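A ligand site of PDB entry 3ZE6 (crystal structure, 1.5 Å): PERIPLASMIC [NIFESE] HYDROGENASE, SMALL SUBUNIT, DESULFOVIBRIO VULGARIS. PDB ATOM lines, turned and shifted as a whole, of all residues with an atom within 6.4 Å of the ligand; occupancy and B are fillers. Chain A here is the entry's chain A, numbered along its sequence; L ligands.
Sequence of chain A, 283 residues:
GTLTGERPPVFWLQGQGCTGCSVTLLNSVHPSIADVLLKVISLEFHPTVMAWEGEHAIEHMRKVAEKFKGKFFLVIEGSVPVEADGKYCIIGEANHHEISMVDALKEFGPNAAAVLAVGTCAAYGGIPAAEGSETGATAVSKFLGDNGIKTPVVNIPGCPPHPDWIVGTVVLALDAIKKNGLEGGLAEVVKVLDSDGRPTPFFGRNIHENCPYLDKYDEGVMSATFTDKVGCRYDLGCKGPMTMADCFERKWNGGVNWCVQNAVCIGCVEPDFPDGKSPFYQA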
ATOM      1  N   ILE A 207      -0.219 -17.980 -26.558  1.00  0.00           N
ATOM      2  CA  ILE A 207       1.171 -18.152 -26.162  1.00  0.00           C
ATOM      3  C   ILE A 207       1.315 -19.174 -25.045  1.00  0.00           C
ATOM      4  O   ILE A 207       2.096 -20.121 -25.159  1.00  0.00           O
ATOM      5  CB  ILE A 207       1.778 -16.824 -25.700  1.00  0.00           C
ATOM      6  CG1 ILE A 207       1.965 -15.903 -26.908  1.00  0.00           C
ATOM      7  CG2 ILE A 207       3.104 -17.052 -25.001  1.00  0.00           C
ATOM      8  CD1 ILE A 207       2.483 -14.548 -26.561  1.00  0.00           C
ATOM      9  N   HIS A 208       0.554 -19.001 -23.972  1.00  0.00           N
ATOM     10  CA  HIS A 208       0.682 -19.816 -22.778  1.00  0.00           C
ATOM     11  C   HIS A 208       0.420 -21.309 -23.041  1.00  0.00           C
ATOM     12  O   HIS A 208       1.163 -22.177 -22.549  1.00  0.00           O
ATOM     13  CB  HIS A 208      -0.290 -19.222 -21.757  1.00  0.00           C
ATOM     14  CG  HIS A 208      -0.453 -20.007 -20.497  1.00  0.00           C
ATOM     15  ND1 HIS A 208       0.478 -20.033 -19.493  1.00  0.00           N
ATOM     16  CD2 HIS A 208      -1.496 -20.770 -20.064  1.00  0.00           C
ATOM     17  CE1 HIS A 208       0.038 -20.777 -18.495  1.00  0.00           C
ATOM     18  NE2 HIS A 208      -1.158 -21.229 -18.816  1.00  0.00           N
ATOM     19  N   GLU A 209      -0.584 -21.611 -23.861  1.00  0.00           N
ATOM     20  CA  GLU A 209      -0.898 -23.017 -24.177  1.00  0.00           C
ATOM     21  C   GLU A 209       0.239 -23.703 -24.906  1.00  0.00           C
ATOM     22  O   GLU A 209       0.353 -24.921 -24.881  1.00  0.00           O
ATOM     23  CB  GLU A 209      -2.186 -23.115 -24.993  1.00  0.00           C
ATOM     24  CG  GLU A 209      -3.421 -22.674 -24.216  1.00  0.00           C
ATOM     25  CD  GLU A 209      -4.682 -22.614 -25.083  1.00  0.00           C
ATOM     26  OE1 GLU A 209      -4.629 -23.039 -26.262  1.00  0.00           O
ATOM     27  OE2 GLU A 209      -5.703 -22.106 -24.573  1.00  0.00           O
ATOM     28  N   CYS A 211       3.582 -22.615 -24.480  1.00  0.00           N
ATOM     29  CA  CYS A 211       4.816 -22.149 -23.842  1.00  0.00           C
ATOM     30  C   CYS A 211       5.686 -23.284 -23.342  1.00  0.00           C
ATOM     31  O   CYS A 211       5.191 -24.223 -22.710  1.00  0.00           O
ATOM     32  CB  CYS A 211       4.487 -21.216 -22.672  1.00  0.00           C
ATOM     33  SG  CYS A 211       5.935 -20.494 -21.896  1.00  0.00           S
ATOM     34  N   PRO A 212       7.008 -23.176 -23.549  1.00  0.00           N
ATOM     35  CA  PRO A 212       7.905 -24.197 -23.017  1.00  0.00           C
ATOM     36  C   PRO A 212       7.969 -24.261 -21.476  1.00  0.00           C
ATOM     37  O   PRO A 212       8.558 -25.205 -20.943  1.00  0.00           O
ATOM     38  CB  PRO A 212       9.279 -23.811 -23.611  1.00  0.00           C
ATOM     39  CG  PRO A 212       9.143 -22.373 -23.948  1.00  0.00           C
ATOM     40  CD  PRO A 212       7.736 -22.133 -24.309  1.00  0.00           C
ATOM     41  N   TYR A 213       7.399 -23.292 -20.761  1.00  0.00           N
ATOM     42  CA  TYR A 213       7.406 -23.278 -19.294  1.00  0.00           C
ATOM     43  C   TYR A 213       6.059 -23.689 -18.711  1.00  0.00           C
ATOM     44  O   TYR A 213       5.854 -23.598 -17.504  1.00  0.00           O
ATOM     45  CB  TYR A 213       7.900 -21.919 -18.741  1.00  0.00           C
ATOM     46  CG  TYR A 213       9.184 -21.499 -19.457  1.00  0.00           C
ATOM     47  CD1 TYR A 213      10.393 -22.151 -19.229  1.00  0.00           C
ATOM     48  CD2 TYR A 213       9.158 -20.478 -20.372  1.00  0.00           C
ATOM     49  CE1 TYR A 213      11.543 -21.761 -19.933  1.00  0.00           C
ATOM     50  CE2 TYR A 213      10.270 -20.097 -21.055  1.00  0.00           C
ATOM     51  CZ  TYR A 213      11.447 -20.727 -20.844  1.00  0.00           C
ATOM     52  OH  TYR A 213      12.536 -20.277 -21.583  1.00  0.00           O
ATOM     53  N   LEU A 214       5.145 -24.144 -19.566  1.00  0.00           N
ATOM     54  CA  LEU A 214       3.789 -24.507 -19.114  1.00  0.00           C
ATOM     55  C   LEU A 214       3.877 -25.631 -18.081  1.00  0.00           C
ATOM     56  O   LEU A 214       3.098 -25.642 -17.116  1.00  0.00           O
ATOM     57  CB  LEU A 214       2.924 -24.921 -20.298  1.00  0.00           C
ATOM     58  CG  LEU A 214       1.450 -25.233 -19.964  1.00  0.00           C
ATOM     59  CD1 LEU A 214       0.728 -24.050 -19.313  1.00  0.00           C
ATOM     60  CD2 LEU A 214       0.741 -25.674 -21.225  1.00  0.00           C
ATOM     61  N   ASP A 215       4.825 -26.547 -18.250  1.00  0.00           N
ATOM     62  CA  ASP A 215       4.978 -27.586 -17.241  1.00  0.00           C
ATOM     63  C   ASP A 215       5.288 -26.999 -15.843  1.00  0.00           C
ATOM     64  O   ASP A 215       4.747 -27.448 -14.830  1.00  0.00           O
ATOM     65  CB  ASP A 215       5.983 -28.678 -17.676  1.00  0.00           C
ATOM     66  CG  ASP A 215       7.410 -28.150 -17.935  1.00  0.00           C
ATOM     67  OD1 ASP A 215       7.624 -26.938 -18.129  1.00  0.00           O
ATOM     68  OD2 ASP A 215       8.341 -28.983 -17.962  1.00  0.00           O
ATOM     69  N   LYS A 216       6.117 -25.959 -15.801  1.00  0.00           N
ATOM     70  CA  LYS A 216       6.448 -25.307 -14.548  1.00  0.00           C
ATOM     71  C   LYS A 216       5.240 -24.555 -13.969  1.00  0.00           C
ATOM     72  O   LYS A 216       4.980 -24.588 -12.773  1.00  0.00           O
ATOM     73  CB  LYS A 216       7.644 -24.381 -14.732  1.00  0.00           C
ATOM     74  CG  LYS A 216       8.891 -25.087 -15.235  1.00  0.00           C
ATOM     75  CD  LYS A 216       9.468 -26.002 -14.154  1.00  0.00           C
ATOM     76  CE  LYS A 216      10.692 -26.775 -14.634  1.00  0.00           C
ATOM     77  NZ  LYS A 216      11.247 -27.623 -13.546  1.00  0.00           N
ATOM     78  N   TYR A 217       4.493 -23.880 -14.831  1.00  0.00           N
ATOM     79  CA  TYR A 217       3.252 -23.259 -14.417  1.00  0.00           C
ATOM     80  C   TYR A 217       2.350 -24.272 -13.735  1.00  0.00           C
ATOM     81  O   TYR A 217       1.802 -23.997 -12.671  1.00  0.00           O
ATOM     82  CB  TYR A 217       2.547 -22.709 -15.661  1.00  0.00           C
ATOM     83  CG  TYR A 217       1.190 -22.073 -15.450  1.00  0.00           C
ATOM     84  CD1 TYR A 217       1.080 -20.721 -15.132  1.00  0.00           C
ATOM     85  CD2 TYR A 217       0.033 -22.823 -15.609  1.00  0.00           C
ATOM     86  CE1 TYR A 217      -0.171 -20.135 -14.988  1.00  0.00           C
ATOM     87  CE2 TYR A 217      -1.190 -22.254 -15.469  1.00  0.00           C
ATOM     88  CZ  TYR A 217      -1.300 -20.929 -15.134  1.00  0.00           C
ATOM     89  OH  TYR A 217      -2.558 -20.407 -14.993  1.00  0.00           O
ATOM     90  N   MET A 222       7.550 -21.157  -9.842  1.00  0.00           N
ATOM     91  CA  MET A 222       7.608 -19.768 -10.320  1.00  0.00           C
ATOM     92  C   MET A 222       8.943 -19.137 -10.014  1.00  0.00           C
ATOM     93  O   MET A 222       9.400 -19.146  -8.873  1.00  0.00           O
ATOM     94  CB  MET A 222       6.559 -18.913  -9.596  1.00  0.00           C
ATOM     95  CG  MET A 222       5.131 -19.319  -9.870  1.00  0.00           C
ATOM     96  SD  MET A 222       4.744 -19.172 -11.616  1.00  0.00           S
ATOM     97  CE  MET A 222       3.195 -20.091 -11.757  1.00  0.00           C
ATOM     98  N   GLY A 231      11.971 -21.396 -13.775  1.00  0.00           N
ATOM     99  CA  GLY A 231      10.572 -21.297 -13.379  1.00  0.00           C
ATOM    100  C   GLY A 231       9.693 -20.616 -14.412  1.00  0.00           C
ATOM    101  O   GLY A 231      10.168 -19.955 -15.340  1.00  0.00           O
ATOM    102  N   CYS A 232       8.399 -20.779 -14.243  1.00  0.00           N
ATOM    103  CA  CYS A 232       7.443 -20.000 -15.022  1.00  0.00           C
ATOM    104  C   CYS A 232       7.512 -18.525 -14.571  1.00  0.00           C
ATOM    105  O   CYS A 232       7.893 -18.199 -13.423  1.00  0.00           O
ATOM    106  CB  CYS A 232       6.035 -20.607 -14.834  1.00  0.00           C
ATOM    107  SG  CYS A 232       4.608 -19.547 -15.206  1.00  0.00           S
ATOM    108  N   ARG A 233       7.150 -17.640 -15.510  1.00  0.00           N
ATOM    109  CA  ARG A 233       7.269 -16.192 -15.340  1.00  0.00           C
ATOM    110  C   ARG A 233       5.946 -15.540 -14.892  1.00  0.00           C
ATOM    111  O   ARG A 233       5.830 -14.314 -14.817  1.00  0.00           O
ATOM    112  CB  ARG A 233       7.721 -15.560 -16.666  1.00  0.00           C
ATOM    113  CG  ARG A 233       9.191 -15.765 -17.068  1.00  0.00           C
ATOM    114  CD  ARG A 233       9.543 -17.203 -17.469  1.00  0.00           C
ATOM    115  NE  ARG A 233      10.749 -17.181 -18.276  1.00  0.00           N
ATOM    116  CZ  ARG A 233      11.674 -18.129 -18.323  1.00  0.00           C
ATOM    117  NH1 ARG A 233      11.602 -19.218 -17.580  1.00  0.00           N
ATOM    118  NH2 ARG A 233      12.705 -17.955 -19.114  1.00  0.00           N
ATOM    119  N   TYR A 234       4.944 -16.343 -14.550  1.00  0.00           N
ATOM    120  CA  TYR A 234       3.632 -15.813 -14.197  1.00  0.00           C
ATOM    121  C   TYR A 234       3.675 -14.816 -13.042  1.00  0.00           C
ATOM    122  O   TYR A 234       3.057 -13.748 -13.116  1.00  0.00           O
ATOM    123  CB  TYR A 234       2.659 -16.976 -13.881  1.00  0.00           C
ATOM    124  CG  TYR A 234       1.296 -16.541 -13.419  1.00  0.00           C
ATOM    125  CD1 TYR A 234       0.308 -16.232 -14.330  1.00  0.00           C
ATOM    126  CD2 TYR A 234       1.019 -16.410 -12.066  1.00  0.00           C
ATOM    127  CE1 TYR A 234      -0.932 -15.818 -13.911  1.00  0.00           C
ATOM    128  CE2 TYR A 234      -0.231 -16.002 -11.637  1.00  0.00           C
ATOM    129  CZ  TYR A 234      -1.193 -15.711 -12.566  1.00  0.00           C
ATOM    130  OH  TYR A 234      -2.450 -15.294 -12.130  1.00  0.00           O
ATOM    131  N   ASP A 235       4.384 -15.123 -11.972  1.00  0.00           N
ATOM    132  CA  ASP A 235       4.449 -14.240 -10.800  1.00  0.00           C
ATOM    133  C   ASP A 235       5.211 -12.944 -11.114  1.00  0.00           C
ATOM    134  O   ASP A 235       4.993 -11.933 -10.459  1.00  0.00           O
ATOM    135  CB  ASP A 235       5.134 -14.899  -9.610  1.00  0.00           C
ATOM    136  CG  ASP A 235       4.278 -15.913  -8.893  1.00  0.00           C
ATOM    137  OD1 ASP A 235       3.070 -16.034  -9.189  1.00  0.00           O
ATOM    138  OD2 ASP A 235       4.871 -16.571  -7.989  1.00  0.00           O
ATOM    139  N   CYS A 238       4.015 -12.233 -16.419  1.00  0.00           N
ATOM    140  CA  CYS A 238       3.806 -12.732 -17.761  1.00  0.00           C
ATOM    141  C   CYS A 238       2.335 -12.780 -18.143  1.00  0.00           C
ATOM    142  O   CYS A 238       1.510 -13.398 -17.427  1.00  0.00           O
ATOM    143  CB  CYS A 238       4.391 -14.148 -17.897  1.00  0.00           C
ATOM    144  SG  CYS A 238       4.346 -14.766 -19.572  1.00  0.00           S
ATOM    145  N   LYS A 239       2.001 -12.170 -19.286  1.00  0.00           N
ATOM    146  CA  LYS A 239       0.629 -12.112 -19.743  1.00  0.00           C
ATOM    147  C   LYS A 239       0.357 -13.129 -20.855  1.00  0.00           C
ATOM    148  O   LYS A 239      -0.674 -13.047 -21.534  1.00  0.00           O
ATOM    149  CB  LYS A 239       0.245 -10.696 -20.199  1.00  0.00           C
ATOM    150  CG  LYS A 239       0.365  -9.639 -19.105  1.00  0.00           C
ATOM    151  CD  LYS A 239      -0.329 -10.036 -17.779  1.00  0.00           C
ATOM    152  CE  LYS A 239      -0.322  -8.871 -16.807  1.00  0.00           C
ATOM    153  NZ  LYS A 239       1.034  -8.288 -16.639  1.00  0.00           N
ATOM    154  N   GLY A 240       1.267 -14.093 -21.035  1.00  0.00           N
ATOM    155  CA  GLY A 240       1.065 -15.148 -22.013  1.00  0.00           C
ATOM    156  C   GLY A 240      -0.328 -15.795 -21.954  1.00  0.00           C
ATOM    157  O   GLY A 240      -0.893 -16.145 -22.974  1.00  0.00           O
ATOM    158  N   PRO A 241      -0.862 -16.023 -20.747  1.00  0.00           N
ATOM    159  CA  PRO A 241      -2.186 -16.663 -20.701  1.00  0.00           C
ATOM    160  C   PRO A 241      -3.291 -15.931 -21.429  1.00  0.00           C
ATOM    161  O   PRO A 241      -4.292 -16.555 -21.812  1.00  0.00           O
ATOM    162  CB  PRO A 241      -2.486 -16.705 -19.203  1.00  0.00           C
ATOM    163  CG  PRO A 241      -1.137 -16.804 -18.567  1.00  0.00           C
ATOM    164  CD  PRO A 241      -0.282 -15.871 -19.408  1.00  0.00           C
ATOM    165  N   TRP A 258      13.149 -14.361 -27.377  1.00  0.00           N
ATOM    166  CA  TRP A 258      11.768 -13.850 -27.341  1.00  0.00           C
ATOM    167  C   TRP A 258      11.412 -13.402 -25.928  1.00  0.00           C
ATOM    168  O   TRP A 258      12.149 -13.643 -24.975  1.00  0.00           O
ATOM    169  CB  TRP A 258      10.767 -14.879 -27.893  1.00  0.00           C
ATOM    170  CG  TRP A 258      10.520 -16.104 -27.081  1.00  0.00           C
ATOM    171  CD1 TRP A 258      11.447 -17.062 -26.710  1.00  0.00           C
ATOM    172  CD2 TRP A 258       9.256 -16.564 -26.575  1.00  0.00           C
ATOM    173  NE1 TRP A 258      10.828 -18.075 -25.986  1.00  0.00           N
ATOM    174  CE2 TRP A 258       9.484 -17.792 -25.900  1.00  0.00           C
ATOM    175  CE3 TRP A 258       7.942 -16.052 -26.624  1.00  0.00           C
ATOM    176  CZ2 TRP A 258       8.447 -18.513 -25.283  1.00  0.00           C
ATOM    177  CZ3 TRP A 258       6.923 -16.782 -26.016  1.00  0.00           C
ATOM    178  CH2 TRP A 258       7.183 -17.985 -25.349  1.00  0.00           C
ATOM    179  N   VAL A 260       9.287 -14.068 -23.486  1.00  0.00           N
ATOM    180  CA  VAL A 260       9.093 -14.951 -22.337  1.00  0.00           C
ATOM    181  C   VAL A 260      10.428 -15.555 -21.890  1.00  0.00           C
ATOM    182  O   VAL A 260      10.690 -15.676 -20.684  1.00  0.00           O
ATOM    183  CB  VAL A 260       8.056 -16.051 -22.654  1.00  0.00           C
ATOM    184  CG1 VAL A 260       7.968 -17.065 -21.524  1.00  0.00           C
ATOM    185  CG2 VAL A 260       6.686 -15.428 -22.908  1.00  0.00           C
ATOM    186  N   CYS A 265       6.116 -11.851 -21.245  1.00  0.00           N
ATOM    187  CA  CYS A 265       5.212 -11.330 -22.270  1.00  0.00           C
ATOM    188  C   CYS A 265       4.353 -10.203 -21.670  1.00  0.00           C
ATOM    189  O   CYS A 265       3.861 -10.363 -20.554  1.00  0.00           O
ATOM    190  CB  CYS A 265       4.325 -12.468 -22.807  1.00  0.00           C
ATOM    191  SG  CYS A 265       3.012 -11.942 -23.952  1.00  0.00           S
HETATM  192 FE1  LIG L   1       4.103 -17.059 -19.206  1.00  0.00          FE
HETATM  193 FE2  LIG L   1       4.371 -19.212 -17.480  1.00  0.00          FE
HETATM  194 FE3  LIG L   1       4.819 -19.482 -20.146  1.00  0.00          FE
HETATM  195 FE4  LIG L   1       2.326 -19.147 -19.261  1.00  0.00          FE
HETATM  196  S1  LIG L   1       3.712 -20.938 -18.808  1.00  0.00           S
HETATM  197  S2  LIG L   1       3.233 -18.058 -21.051  1.00  0.00           S
HETATM  198  S3  LIG L   1       2.651 -17.675 -17.539  1.00  0.00           S
HETATM  199  S4  LIG L   1       6.050 -18.202 -18.673  1.00  0.00           S
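The side-chain sulfur (SG) of Cys 238 is bound to an iron atom (FE1) of the ligand (2.3 Å).
FE3 of the ligand is bound by SG of Cys 211, at 2.3 Å.
The backbone NH of Arg 233 sits close to a sulfur (S4) of the ligand, at 3.4 Å.
FE2 of the ligand is bound by SG of Cys 232.
A ring nitrogen (ND1) of His 208 binds an iron atom (FE4) of the ligand (2.1 Å).
N of Leu 214 lies close to S1 of the ligand (3.6 Å).
The backbone carbonyl oxygen (O) of Tyr 213 sits close to a sulfur (S1) of the ligand (3.7 Å).
CB of Tyr 217 touches S1 of the ligand (3.8 Å).
Tyr 234 touches the ligand (CB to S3, 3.7 Å).
Gly 240 touches the ligand.
Pro 241 touches the ligand (CD to S3, 3.9 Å).
Val 260 touches the ligand.
Hydrophobic or aromatic side chains within 4 Å of the ligand: His 208, Tyr 217, Tyr 234, Pro 241 and Val 260.
The side-chain sulfur (SG) of Cys 238 lies close to the backbone NH (N) of Gly 240 (3.5 Å).
N of Cys 238 sits at hydrogen-bond distance from O of Arg 233 (3.2 Å).
The side-chain sulfur of Cys 232 lies close to the side-chain sulfur of Met 222, 3.6 Å away.
The backbone carbonyl oxygen (O) of Gly 231 is in hydrogen-bond range of the guanidinium group (NH1) of Arg 233 (2.8 Å).
The backbone NH (N) of Tyr 234 lies close to the side-chain sulfur (SG) of Cys 232.
The backbone NH of Cys 265 lies close to the side-chain sulfur of Cys 238.
NH2 of Arg 233 is in hydrogen-bond range of OH of Tyr 213.
NE of Arg 233 is in hydrogen-bond range of O of Val 260 (2.8 Å).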
